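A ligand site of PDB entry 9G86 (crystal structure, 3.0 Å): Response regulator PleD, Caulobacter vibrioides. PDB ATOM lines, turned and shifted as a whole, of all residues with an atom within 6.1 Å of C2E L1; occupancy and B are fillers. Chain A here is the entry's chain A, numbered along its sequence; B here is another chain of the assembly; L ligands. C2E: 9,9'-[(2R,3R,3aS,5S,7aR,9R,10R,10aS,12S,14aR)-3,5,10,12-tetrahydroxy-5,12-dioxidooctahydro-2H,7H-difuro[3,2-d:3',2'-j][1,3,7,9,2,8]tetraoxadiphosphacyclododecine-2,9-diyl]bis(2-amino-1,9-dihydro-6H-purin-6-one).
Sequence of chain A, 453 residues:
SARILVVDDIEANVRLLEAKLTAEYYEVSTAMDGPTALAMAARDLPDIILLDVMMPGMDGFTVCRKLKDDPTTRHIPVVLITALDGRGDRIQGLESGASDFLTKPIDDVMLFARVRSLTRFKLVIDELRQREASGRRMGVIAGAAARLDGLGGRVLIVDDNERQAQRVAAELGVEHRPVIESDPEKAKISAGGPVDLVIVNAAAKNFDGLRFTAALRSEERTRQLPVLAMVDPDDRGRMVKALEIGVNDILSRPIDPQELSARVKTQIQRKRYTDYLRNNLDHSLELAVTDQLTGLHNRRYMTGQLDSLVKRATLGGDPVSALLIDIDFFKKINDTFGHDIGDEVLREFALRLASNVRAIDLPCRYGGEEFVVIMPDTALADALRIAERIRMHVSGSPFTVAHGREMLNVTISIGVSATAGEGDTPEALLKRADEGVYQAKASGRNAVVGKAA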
ATOM      1  N   ASN A 356     -14.990   8.197  -8.155  1.00  0.00           N
ATOM      2  CA  ASN A 356     -13.758   8.689  -7.553  1.00  0.00           C
ATOM      3  C   ASN A 356     -13.993   9.614  -6.361  1.00  0.00           C
ATOM      4  O   ASN A 356     -13.041  10.231  -5.869  1.00  0.00           O
ATOM      5  CB  ASN A 356     -12.906   9.377  -8.617  1.00  0.00           C
ATOM      6  CG  ASN A 356     -12.335   8.403  -9.625  1.00  0.00           C
ATOM      7  OD1 ASN A 356     -11.352   7.711  -9.351  1.00  0.00           O
ATOM      8  ND2 ASN A 356     -12.973   8.304 -10.778  1.00  0.00           N
ATOM      9  N   VAL A 357     -15.241   9.719  -5.878  1.00  0.00           N
ATOM     10  CA  VAL A 357     -15.548  10.395  -4.627  1.00  0.00           C
ATOM     11  C   VAL A 357     -16.364   9.440  -3.765  1.00  0.00           C
ATOM     12  O   VAL A 357     -16.945   8.465  -4.247  1.00  0.00           O
ATOM     13  CB  VAL A 357     -16.308  11.729  -4.808  1.00  0.00           C
ATOM     14  CG1 VAL A 357     -15.523  12.668  -5.691  1.00  0.00           C
ATOM     15  CG2 VAL A 357     -17.694  11.469  -5.362  1.00  0.00           C
ATOM     16  N   ARG A 358     -16.423   9.748  -2.468  1.00  0.00           N
ATOM     17  CA  ARG A 358     -17.093   8.868  -1.527  1.00  0.00           C
ATOM     18  C   ARG A 358     -18.597   8.856  -1.778  1.00  0.00           C
ATOM     19  O   ARG A 358     -19.156   9.785  -2.350  1.00  0.00           O
ATOM     20  CB  ARG A 358     -16.813   9.312  -0.088  1.00  0.00           C
ATOM     21  CG  ARG A 358     -15.420   8.962   0.404  1.00  0.00           C
ATOM     22  CD  ARG A 358     -15.131   9.549   1.780  1.00  0.00           C
ATOM     23  NE  ARG A 358     -13.713   9.428   2.103  1.00  0.00           N
ATOM     24  CZ  ARG A 358     -13.171   9.738   3.269  1.00  0.00           C
ATOM     25  NH1 ARG A 358     -13.906  10.258   4.255  1.00  0.00           N
ATOM     26  NH2 ARG A 358     -11.875   9.526   3.465  1.00  0.00           N
ATOM     27  N   ILE A 360     -20.707   8.941   0.628  1.00  0.00           N
ATOM     28  CA  ILE A 360     -21.263   9.915   1.557  1.00  0.00           C
ATOM     29  C   ILE A 360     -21.263  11.299   0.941  1.00  0.00           C
ATOM     30  O   ILE A 360     -21.999  12.180   1.391  1.00  0.00           O
ATOM     31  CB  ILE A 360     -20.512   9.895   2.896  1.00  0.00           C
ATOM     32  CG1 ILE A 360     -19.055  10.335   2.727  1.00  0.00           C
ATOM     33  CG2 ILE A 360     -20.575   8.504   3.504  1.00  0.00           C
ATOM     34  CD1 ILE A 360     -18.784  11.745   3.251  1.00  0.00           C
ATOM     35  N   ASP A 361     -20.428  11.519  -0.080  1.00  0.00           N
ATOM     36  CA  ASP A 361     -20.464  12.775  -0.819  1.00  0.00           C
ATOM     37  C   ASP A 361     -21.688  12.802  -1.726  1.00  0.00           C
ATOM     38  O   ASP A 361     -22.374  11.803  -1.927  1.00  0.00           O
ATOM     39  CB  ASP A 361     -19.184  12.953  -1.644  1.00  0.00           C
ATOM     40  CG  ASP A 361     -17.908  12.854  -0.819  1.00  0.00           C
ATOM     41  OD1 ASP A 361     -17.957  13.148   0.397  1.00  0.00           O
ATOM     42  OD2 ASP A 361     -16.866  12.491  -1.389  1.00  0.00           O
ATOM     43  N   MET A 375     -19.130  17.702  -0.482  1.00  0.00           N
ATOM     44  CA  MET A 375     -18.423  16.768   0.385  1.00  0.00           C
ATOM     45  C   MET A 375     -18.659  17.131   1.851  1.00  0.00           C
ATOM     46  O   MET A 375     -18.175  18.180   2.307  1.00  0.00           O
ATOM     47  CB  MET A 375     -16.937  16.754   0.064  1.00  0.00           C
ATOM     48  CG  MET A 375     -16.560  16.095  -1.248  1.00  0.00           C
ATOM     49  SD  MET A 375     -14.866  16.520  -1.692  1.00  0.00           S
ATOM     50  CE  MET A 375     -14.904  18.277  -1.379  1.00  0.00           C
ATOM     51  N   PRO A 376     -19.432  16.340   2.588  1.00  0.00           N
ATOM     52  CA  PRO A 376     -19.644  16.633   4.015  1.00  0.00           C
ATOM     53  C   PRO A 376     -18.413  16.359   4.848  1.00  0.00           C
ATOM     54  O   PRO A 376     -17.572  15.514   4.516  1.00  0.00           O
ATOM     55  CB  PRO A 376     -20.799  15.690   4.407  1.00  0.00           C
ATOM     56  CG  PRO A 376     -21.383  15.205   3.103  1.00  0.00           C
ATOM     57  CD  PRO A 376     -20.230  15.180   2.156  1.00  0.00           C
ATOM     58  N   ASP A 377     -18.295  17.107   5.940  1.00  0.00           N
ATOM     59  CA  ASP A 377     -17.255  16.950   6.962  1.00  0.00           C
ATOM     60  C   ASP A 377     -15.844  16.876   6.363  1.00  0.00           C
ATOM     61  O   ASP A 377     -15.067  15.957   6.646  1.00  0.00           O
ATOM     62  CB  ASP A 377     -17.521  15.708   7.819  1.00  0.00           C
ATOM     63  CG  ASP A 377     -18.914  15.700   8.419  1.00  0.00           C
ATOM     64  OD1 ASP A 377     -19.388  16.769   8.855  1.00  0.00           O
ATOM     65  OD2 ASP A 377     -19.536  14.610   8.474  1.00  0.00           O
ATOM     66  N   THR A 378     -15.495  17.873   5.550  1.00  0.00           N
ATOM     67  CA  THR A 378     -14.167  17.939   4.954  1.00  0.00           C
ATOM     68  C   THR A 378     -13.672  19.382   4.932  1.00  0.00           C
ATOM     69  O   THR A 378     -14.461  20.323   4.825  1.00  0.00           O
ATOM     70  CB  THR A 378     -14.147  17.337   3.546  1.00  0.00           C
ATOM     71  OG1 THR A 378     -12.865  17.579   2.935  1.00  0.00           O
ATOM     72  CG2 THR A 378     -15.211  17.954   2.719  1.00  0.00           C
ATOM     73  N   ASP A 382      -8.052  19.322   2.040  1.00  0.00           N
ATOM     74  CA  ASP A 382      -8.374  17.982   1.566  1.00  0.00           C
ATOM     75  C   ASP A 382      -9.272  18.064   0.332  1.00  0.00           C
ATOM     76  O   ASP A 382      -9.127  17.264  -0.598  1.00  0.00           O
ATOM     77  CB  ASP A 382      -9.040  17.173   2.670  1.00  0.00           C
ATOM     78  CG  ASP A 382      -8.076  16.766   3.770  1.00  0.00           C
ATOM     79  OD1 ASP A 382      -6.907  16.450   3.451  1.00  0.00           O
ATOM     80  OD2 ASP A 382      -8.479  16.738   4.954  1.00  0.00           O
ATOM     81  N   ALA A 383     -10.216  19.009   0.335  1.00  0.00           N
ATOM     82  CA  ALA A 383     -11.096  19.186  -0.814  1.00  0.00           C
ATOM     83  C   ALA A 383     -10.299  19.510  -2.082  1.00  0.00           C
ATOM     84  O   ALA A 383     -10.603  18.986  -3.156  1.00  0.00           O
ATOM     85  CB  ALA A 383     -12.097  20.307  -0.516  1.00  0.00           C
ATOM     86  N   ARG A 385      -7.212  18.654  -2.681  1.00  0.00           N
ATOM     87  CA  ARG A 385      -6.516  17.436  -3.109  1.00  0.00           C
ATOM     88  C   ARG A 385      -7.484  16.482  -3.823  1.00  0.00           C
ATOM     89  O   ARG A 385      -7.115  15.835  -4.813  1.00  0.00           O
ATOM     90  CB  ARG A 385      -5.856  16.740  -1.929  1.00  0.00           C
ATOM     91  CG  ARG A 385      -5.007  17.612  -1.015  1.00  0.00           C
ATOM     92  CD  ARG A 385      -4.563  16.856   0.242  1.00  0.00           C
ATOM     93  NE  ARG A 385      -5.674  16.154   0.880  1.00  0.00           N
ATOM     94  CZ  ARG A 385      -5.929  14.851   0.743  1.00  0.00           C
ATOM     95  NH1 ARG A 385      -5.134  14.064   0.043  1.00  0.00           N
ATOM     96  NH2 ARG A 385      -7.006  14.336   1.318  1.00  0.00           N
ATOM     97  N   ILE A 386      -8.717  16.375  -3.316  1.00  0.00           N
ATOM     98  CA  ILE A 386      -9.718  15.544  -3.970  1.00  0.00           C
ATOM     99  C   ILE A 386     -10.023  16.064  -5.366  1.00  0.00           C
ATOM    100  O   ILE A 386     -10.186  15.296  -6.326  1.00  0.00           O
ATOM    101  CB  ILE A 386     -10.993  15.449  -3.109  1.00  0.00           C
ATOM    102  CG1 ILE A 386     -10.681  14.897  -1.724  1.00  0.00           C
ATOM    103  CG2 ILE A 386     -12.039  14.583  -3.789  1.00  0.00           C
ATOM    104  CD1 ILE A 386     -11.663  15.353  -0.670  1.00  0.00           C
ATOM    105  N   ARG A 389      -7.426  14.884  -7.577  1.00  0.00           N
ATOM    106  CA  ARG A 389      -7.669  13.481  -7.915  1.00  0.00           C
ATOM    107  C   ARG A 389      -8.676  13.367  -9.057  1.00  0.00           C
ATOM    108  O   ARG A 389      -8.440  12.659 -10.048  1.00  0.00           O
ATOM    109  CB  ARG A 389      -8.125  12.716  -6.671  1.00  0.00           C
ATOM    110  CG  ARG A 389      -8.544  11.273  -6.909  1.00  0.00           C
ATOM    111  CD  ARG A 389      -8.837  10.522  -5.614  1.00  0.00           C
ATOM    112  NE  ARG A 389     -10.135  10.813  -5.012  1.00  0.00           N
ATOM    113  CZ  ARG A 389     -10.302  11.223  -3.753  1.00  0.00           C
ATOM    114  NH1 ARG A 389      -9.283  11.542  -2.984  1.00  0.00           N
ATOM    115  NH2 ARG A 389     -11.541  11.310  -3.268  1.00  0.00           N
ATOM    116  N   ARG B 177     -18.702   5.291   7.255  1.00  0.00           N
ATOM    117  CA  ARG B 177     -18.228   6.625   7.597  1.00  0.00           C
ATOM    118  C   ARG B 177     -19.033   7.152   8.782  1.00  0.00           C
ATOM    119  O   ARG B 177     -20.170   7.626   8.596  1.00  0.00           O
ATOM    120  CB  ARG B 177     -18.349   7.545   6.384  1.00  0.00           C
ATOM    121  CG  ARG B 177     -17.853   6.910   5.099  1.00  0.00           C
ATOM    122  CD  ARG B 177     -16.346   6.954   4.944  1.00  0.00           C
ATOM    123  NE  ARG B 177     -15.956   6.552   3.597  1.00  0.00           N
ATOM    124  CZ  ARG B 177     -14.710   6.343   3.203  1.00  0.00           C
ATOM    125  NH1 ARG B 177     -13.713   6.284   4.070  1.00  0.00           N
ATOM    126  NH2 ARG B 177     -14.456   6.158   1.909  1.00  0.00           N
HETATM  127  P1  C2E L   1      -6.124  10.927   2.284  1.00  0.00           P
HETATM  128  O2P C2E L   1      -5.064  12.016   2.415  1.00  0.00           O
HETATM  129  O1P C2E L   1      -6.273  10.672   0.801  1.00  0.00           O
HETATM  130  O5' C2E L   1      -7.497  11.529   3.038  1.00  0.00           O
HETATM  131  C5' C2E L   1      -7.312  12.513   4.068  1.00  0.00           C
HETATM  132  C4' C2E L   1      -8.707  13.053   4.488  1.00  0.00           C
HETATM  133  O4' C2E L   1      -9.340  13.843   3.226  1.00  0.00           O
HETATM  134  C3' C2E L   1      -9.511  12.116   4.726  1.00  0.00           C
HETATM  135  O3' C2E L   1      -9.422  11.725   6.229  1.00  0.00           O
HETATM  136  C2' C2E L   1     -10.914  12.715   4.350  1.00  0.00           C
HETATM  137  O2' C2E L   1     -11.459  13.395   5.402  1.00  0.00           O
HETATM  138  C1' C2E L   1     -10.629  13.629   3.187  1.00  0.00           C
HETATM  139  N9  C2E L   1     -10.940  12.907   1.902  1.00  0.00           N
HETATM  140  C8  C2E L   1     -10.211  12.206   1.029  1.00  0.00           C
HETATM  141  N7  C2E L   1     -11.084  11.784   0.080  1.00  0.00           N
HETATM  142  C5  C2E L   1     -12.306  12.208   0.399  1.00  0.00           C
HETATM  143  C6  C2E L   1     -13.668  12.035  -0.288  1.00  0.00           C
HETATM  144  O6  C2E L   1     -13.751  11.421  -1.299  1.00  0.00           O
HETATM  145  N1  C2E L   1     -14.832  12.609   0.297  1.00  0.00           N
HETATM  146  C2  C2E L   1     -14.722  13.354   1.523  1.00  0.00           C
HETATM  147  N2  C2E L   1     -15.900  13.945   2.126  1.00  0.00           N
HETATM  148  N3  C2E L   1     -13.433  13.524   2.188  1.00  0.00           N
HETATM  149  C4  C2E L   1     -12.236  12.907   1.568  1.00  0.00           C
HETATM  150  P11 C2E L   1      -9.727  10.047   6.486  1.00  0.00           P
HETATM  151  O21 C2E L   1      -9.060   9.733   7.814  1.00  0.00           O
HETATM  152  O11 C2E L   1     -11.161   9.590   6.577  1.00  0.00           O
HETATM  153  O5A C2E L   1      -8.785   9.350   5.281  1.00  0.00           O
HETATM  154  C5A C2E L   1      -7.398   9.092   5.723  1.00  0.00           C
HETATM  155  C4A C2E L   1      -6.688   8.222   4.668  1.00  0.00           C
HETATM  156  O4A C2E L   1      -7.438   6.773   4.591  1.00  0.00           O
HETATM  157  C3A C2E L   1      -6.783   8.706   3.502  1.00  0.00           C
HETATM  158  O3A C2E L   1      -5.555   9.597   3.141  1.00  0.00           O
HETATM  159  C2A C2E L   1      -6.775   7.474   2.538  1.00  0.00           C
HETATM  160  O2A C2E L   1      -5.497   7.089   2.239  1.00  0.00           O
HETATM  161  C1A C2E L   1      -7.468   6.405   3.337  1.00  0.00           C
HETATM  162  N91 C2E L   1      -8.893   6.215   2.902  1.00  0.00           N
HETATM  163  C81 C2E L   1     -10.036   6.462   3.560  1.00  0.00           C
HETATM  164  N71 C2E L   1     -11.049   6.097   2.739  1.00  0.00           N
HETATM  165  C51 C2E L   1     -10.525   5.632   1.607  1.00  0.00           C
HETATM  166  C61 C2E L   1     -11.177   5.084   0.320  1.00  0.00           C
HETATM  167  O61 C2E L   1     -12.357   5.015   0.228  1.00  0.00           O
HETATM  168  N11 C2E L   1     -10.354   4.640  -0.761  1.00  0.00           N
HETATM  169  C21 C2E L   1      -8.923   4.717  -0.633  1.00  0.00           C
HETATM  170  N21 C2E L   1      -8.099   4.261  -1.735  1.00  0.00           N
HETATM  171  N31 C2E L   1      -8.301   5.234   0.580  1.00  0.00           N
HETATM  172  C41 C2E L   1      -9.164   5.685   1.701  1.00  0.00           C
HETATM  173  P1  C2E L   2     -11.799   2.703  -3.589  1.00  0.00           P
HETATM  174  O2P C2E L   2     -11.815   1.429  -4.416  1.00  0.00           O
HETATM  175  O1P C2E L   2     -10.356   2.964  -3.207  1.00  0.00           O
HETATM  176  O5' C2E L   2     -12.749   2.369  -2.264  1.00  0.00           O
HETATM  177  C5' C2E L   2     -13.843   1.448  -2.439  1.00  0.00           C
HETATM  178  C4' C2E L   2     -14.845   1.639  -1.280  1.00  0.00           C
HETATM  179  O4' C2E L   2     -14.245   0.870   0.015  1.00  0.00           O
HETATM  180  C3' C2E L   2     -14.983   2.853  -0.953  1.00  0.00           C
HETATM  181  O3' C2E L   2     -16.253   3.445  -1.613  1.00  0.00           O
HETATM  182  C2' C2E L   2     -15.192   2.826   0.594  1.00  0.00           C
HETATM  183  O2' C2E L   2     -16.513   2.638   0.892  1.00  0.00           O
HETATM  184  C1' C2E L   2     -14.417   1.623   1.060  1.00  0.00           C
HETATM  185  N9  C2E L   2     -13.088   2.006   1.675  1.00  0.00           N
HETATM  186  C8  C2E L   2     -11.817   1.985   1.278  1.00  0.00           C
HETATM  187  N7  C2E L   2     -11.088   2.460   2.333  1.00  0.00           N
HETATM  188  C5  C2E L   2     -11.933   2.743   3.335  1.00  0.00           C
HETATM  189  C6  C2E L   2     -11.689   3.302   4.749  1.00  0.00           C
HETATM  190  O6  C2E L   2     -10.593   3.566   5.119  1.00  0.00           O
HETATM  191  N1  C2E L   2     -12.811   3.510   5.611  1.00  0.00           N
HETATM  192  C2  C2E L   2     -14.148   3.203   5.154  1.00  0.00           C
HETATM  193  N2  C2E L   2     -15.273   3.411   6.025  1.00  0.00           N
HETATM  194  N3  C2E L   2     -14.374   2.672   3.821  1.00  0.00           N
HETATM  195  C4  C2E L   2     -13.203   2.461   2.921  1.00  0.00           C
HETATM  196  P11 C2E L   2     -16.311   5.154  -1.487  1.00  0.00           P
HETATM  197  O21 C2E L   2     -17.441   5.588  -2.406  1.00  0.00           O
HETATM  198  O11 C2E L   2     -16.575   5.738  -0.123  1.00  0.00           O
HETATM  199  O5A C2E L   2     -14.870   5.647  -2.214  1.00  0.00           O
HETATM  200  C5A C2E L   2     -14.979   5.601  -3.673  1.00  0.00           C
HETATM  201  C4A C2E L   2     -13.591   5.891  -4.291  1.00  0.00           C
HETATM  202  O4A C2E L   2     -13.191   7.423  -3.950  1.00  0.00           O
HETATM  203  C3A C2E L   2     -12.674   5.178  -3.787  1.00  0.00           C
HETATM  204  O3A C2E L   2     -12.467   3.874  -4.610  1.00  0.00           O
HETATM  205  C2A C2E L   2     -11.391   6.060  -3.913  1.00  0.00           C
HETATM  206  O2A C2E L   2     -10.862   5.973  -5.169  1.00  0.00           O
HETATM  207  C1A C2E L   2     -11.918   7.462  -3.674  1.00  0.00           C
HETATM  208  N91 C2E L   2     -11.760   7.818  -2.224  1.00  0.00           N
HETATM  209  C81 C2E L   2     -12.678   7.789  -1.240  1.00  0.00           C
HETATM  210  N71 C2E L   2     -12.055   8.198  -0.116  1.00  0.00           N
HETATM  211  C51 C2E L   2     -10.782   8.476  -0.403  1.00  0.00           C
HETATM  212  C61 C2E L   2      -9.627   8.967   0.469  1.00  0.00           C
HETATM  213  O61 C2E L   2      -9.782   9.185   1.627  1.00  0.00           O
HETATM  214  N11 C2E L   2      -8.341   9.180  -0.111  1.00  0.00           N
HETATM  215  C21 C2E L   2      -8.146   8.926  -1.510  1.00  0.00           C
HETATM  216  N21 C2E L   2      -6.831   9.143  -2.080  1.00  0.00           N
HETATM  217  N31 C2E L   2      -9.249   8.451  -2.354  1.00  0.00           N
HETATM  218  C41 C2E L   2     -10.588   8.227  -1.739  1.00  0.00           C
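NH2 of Arg 177 of chain B is in hydrogen-bond range of O61 of C2E L1, 2.9 Å away. N of Arg 358 is in hydrogen-bond range of O6 of C2E L1, at 3.4 Å. O of Pro 376 lies within hydrogen-bond range of N2 of C2E L1, 3.3 Å away. NH2 of Arg 358 lies within hydrogen-bond range of O61 of C2E L2, at 2.8 Å. N31 of C2E L2 sits at hydrogen-bond distance from NH1 of Arg 389, at 3.2 Å. NH1 of Arg 385 is in salt-bridge range of O2P of C2E L1, 3.1 Å away. The side-chain carboxylate (OD2) of Asp 361 sits at hydrogen-bond distance from a nitrogen (N1) of C2E L1 (2.6 Å). O11 of C2E L1 lies within salt-bridge range of NH2 of Arg 358. The guanidinium group of Arg 389 sits at hydrogen-bond distance from an oxygen (O6) of C2E L1, at 3.0 Å. An oxygen (O11) of C2E L2 lies within salt-bridge range of the guanidinium group (NH2) of Arg 177 of chain B (3.0 Å).
An oxygen (O1P) of C2E L1 lies within hydrogen-bond range of a nitrogen (N11) of C2E L2 (2.7 Å).
The guanidinium group of Arg 385 lies within salt-bridge range of the side-chain carboxylate of Asp 382 (2.9 Å). The backbone carbonyl oxygen (O) of Asn 356 lies within hydrogen-bond range of the guanidinium group (NE) of Arg 389 (3.1 Å). The side-chain carboxylate of Asp 361 lies within hydrogen-bond range of the backbone NH of Arg 358 (3.0 Å).
O4' of C2E L1 sits close to OD2 of Asp 382, 3.5 Å away. CA of Val 357 touches O6 of C2E L1, at 3.9 Å. CD1 of Ile 360 touches N2 of C2E L1 (3.8 Å). Met 375 touches C2E L1 (CB to N2, 3.6 Å). Ile 386 touches C2E L1 (CD1 to C4, 3.4 Å). Of the 15 residues printed, 11 come within 4 Å of C2E L1.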
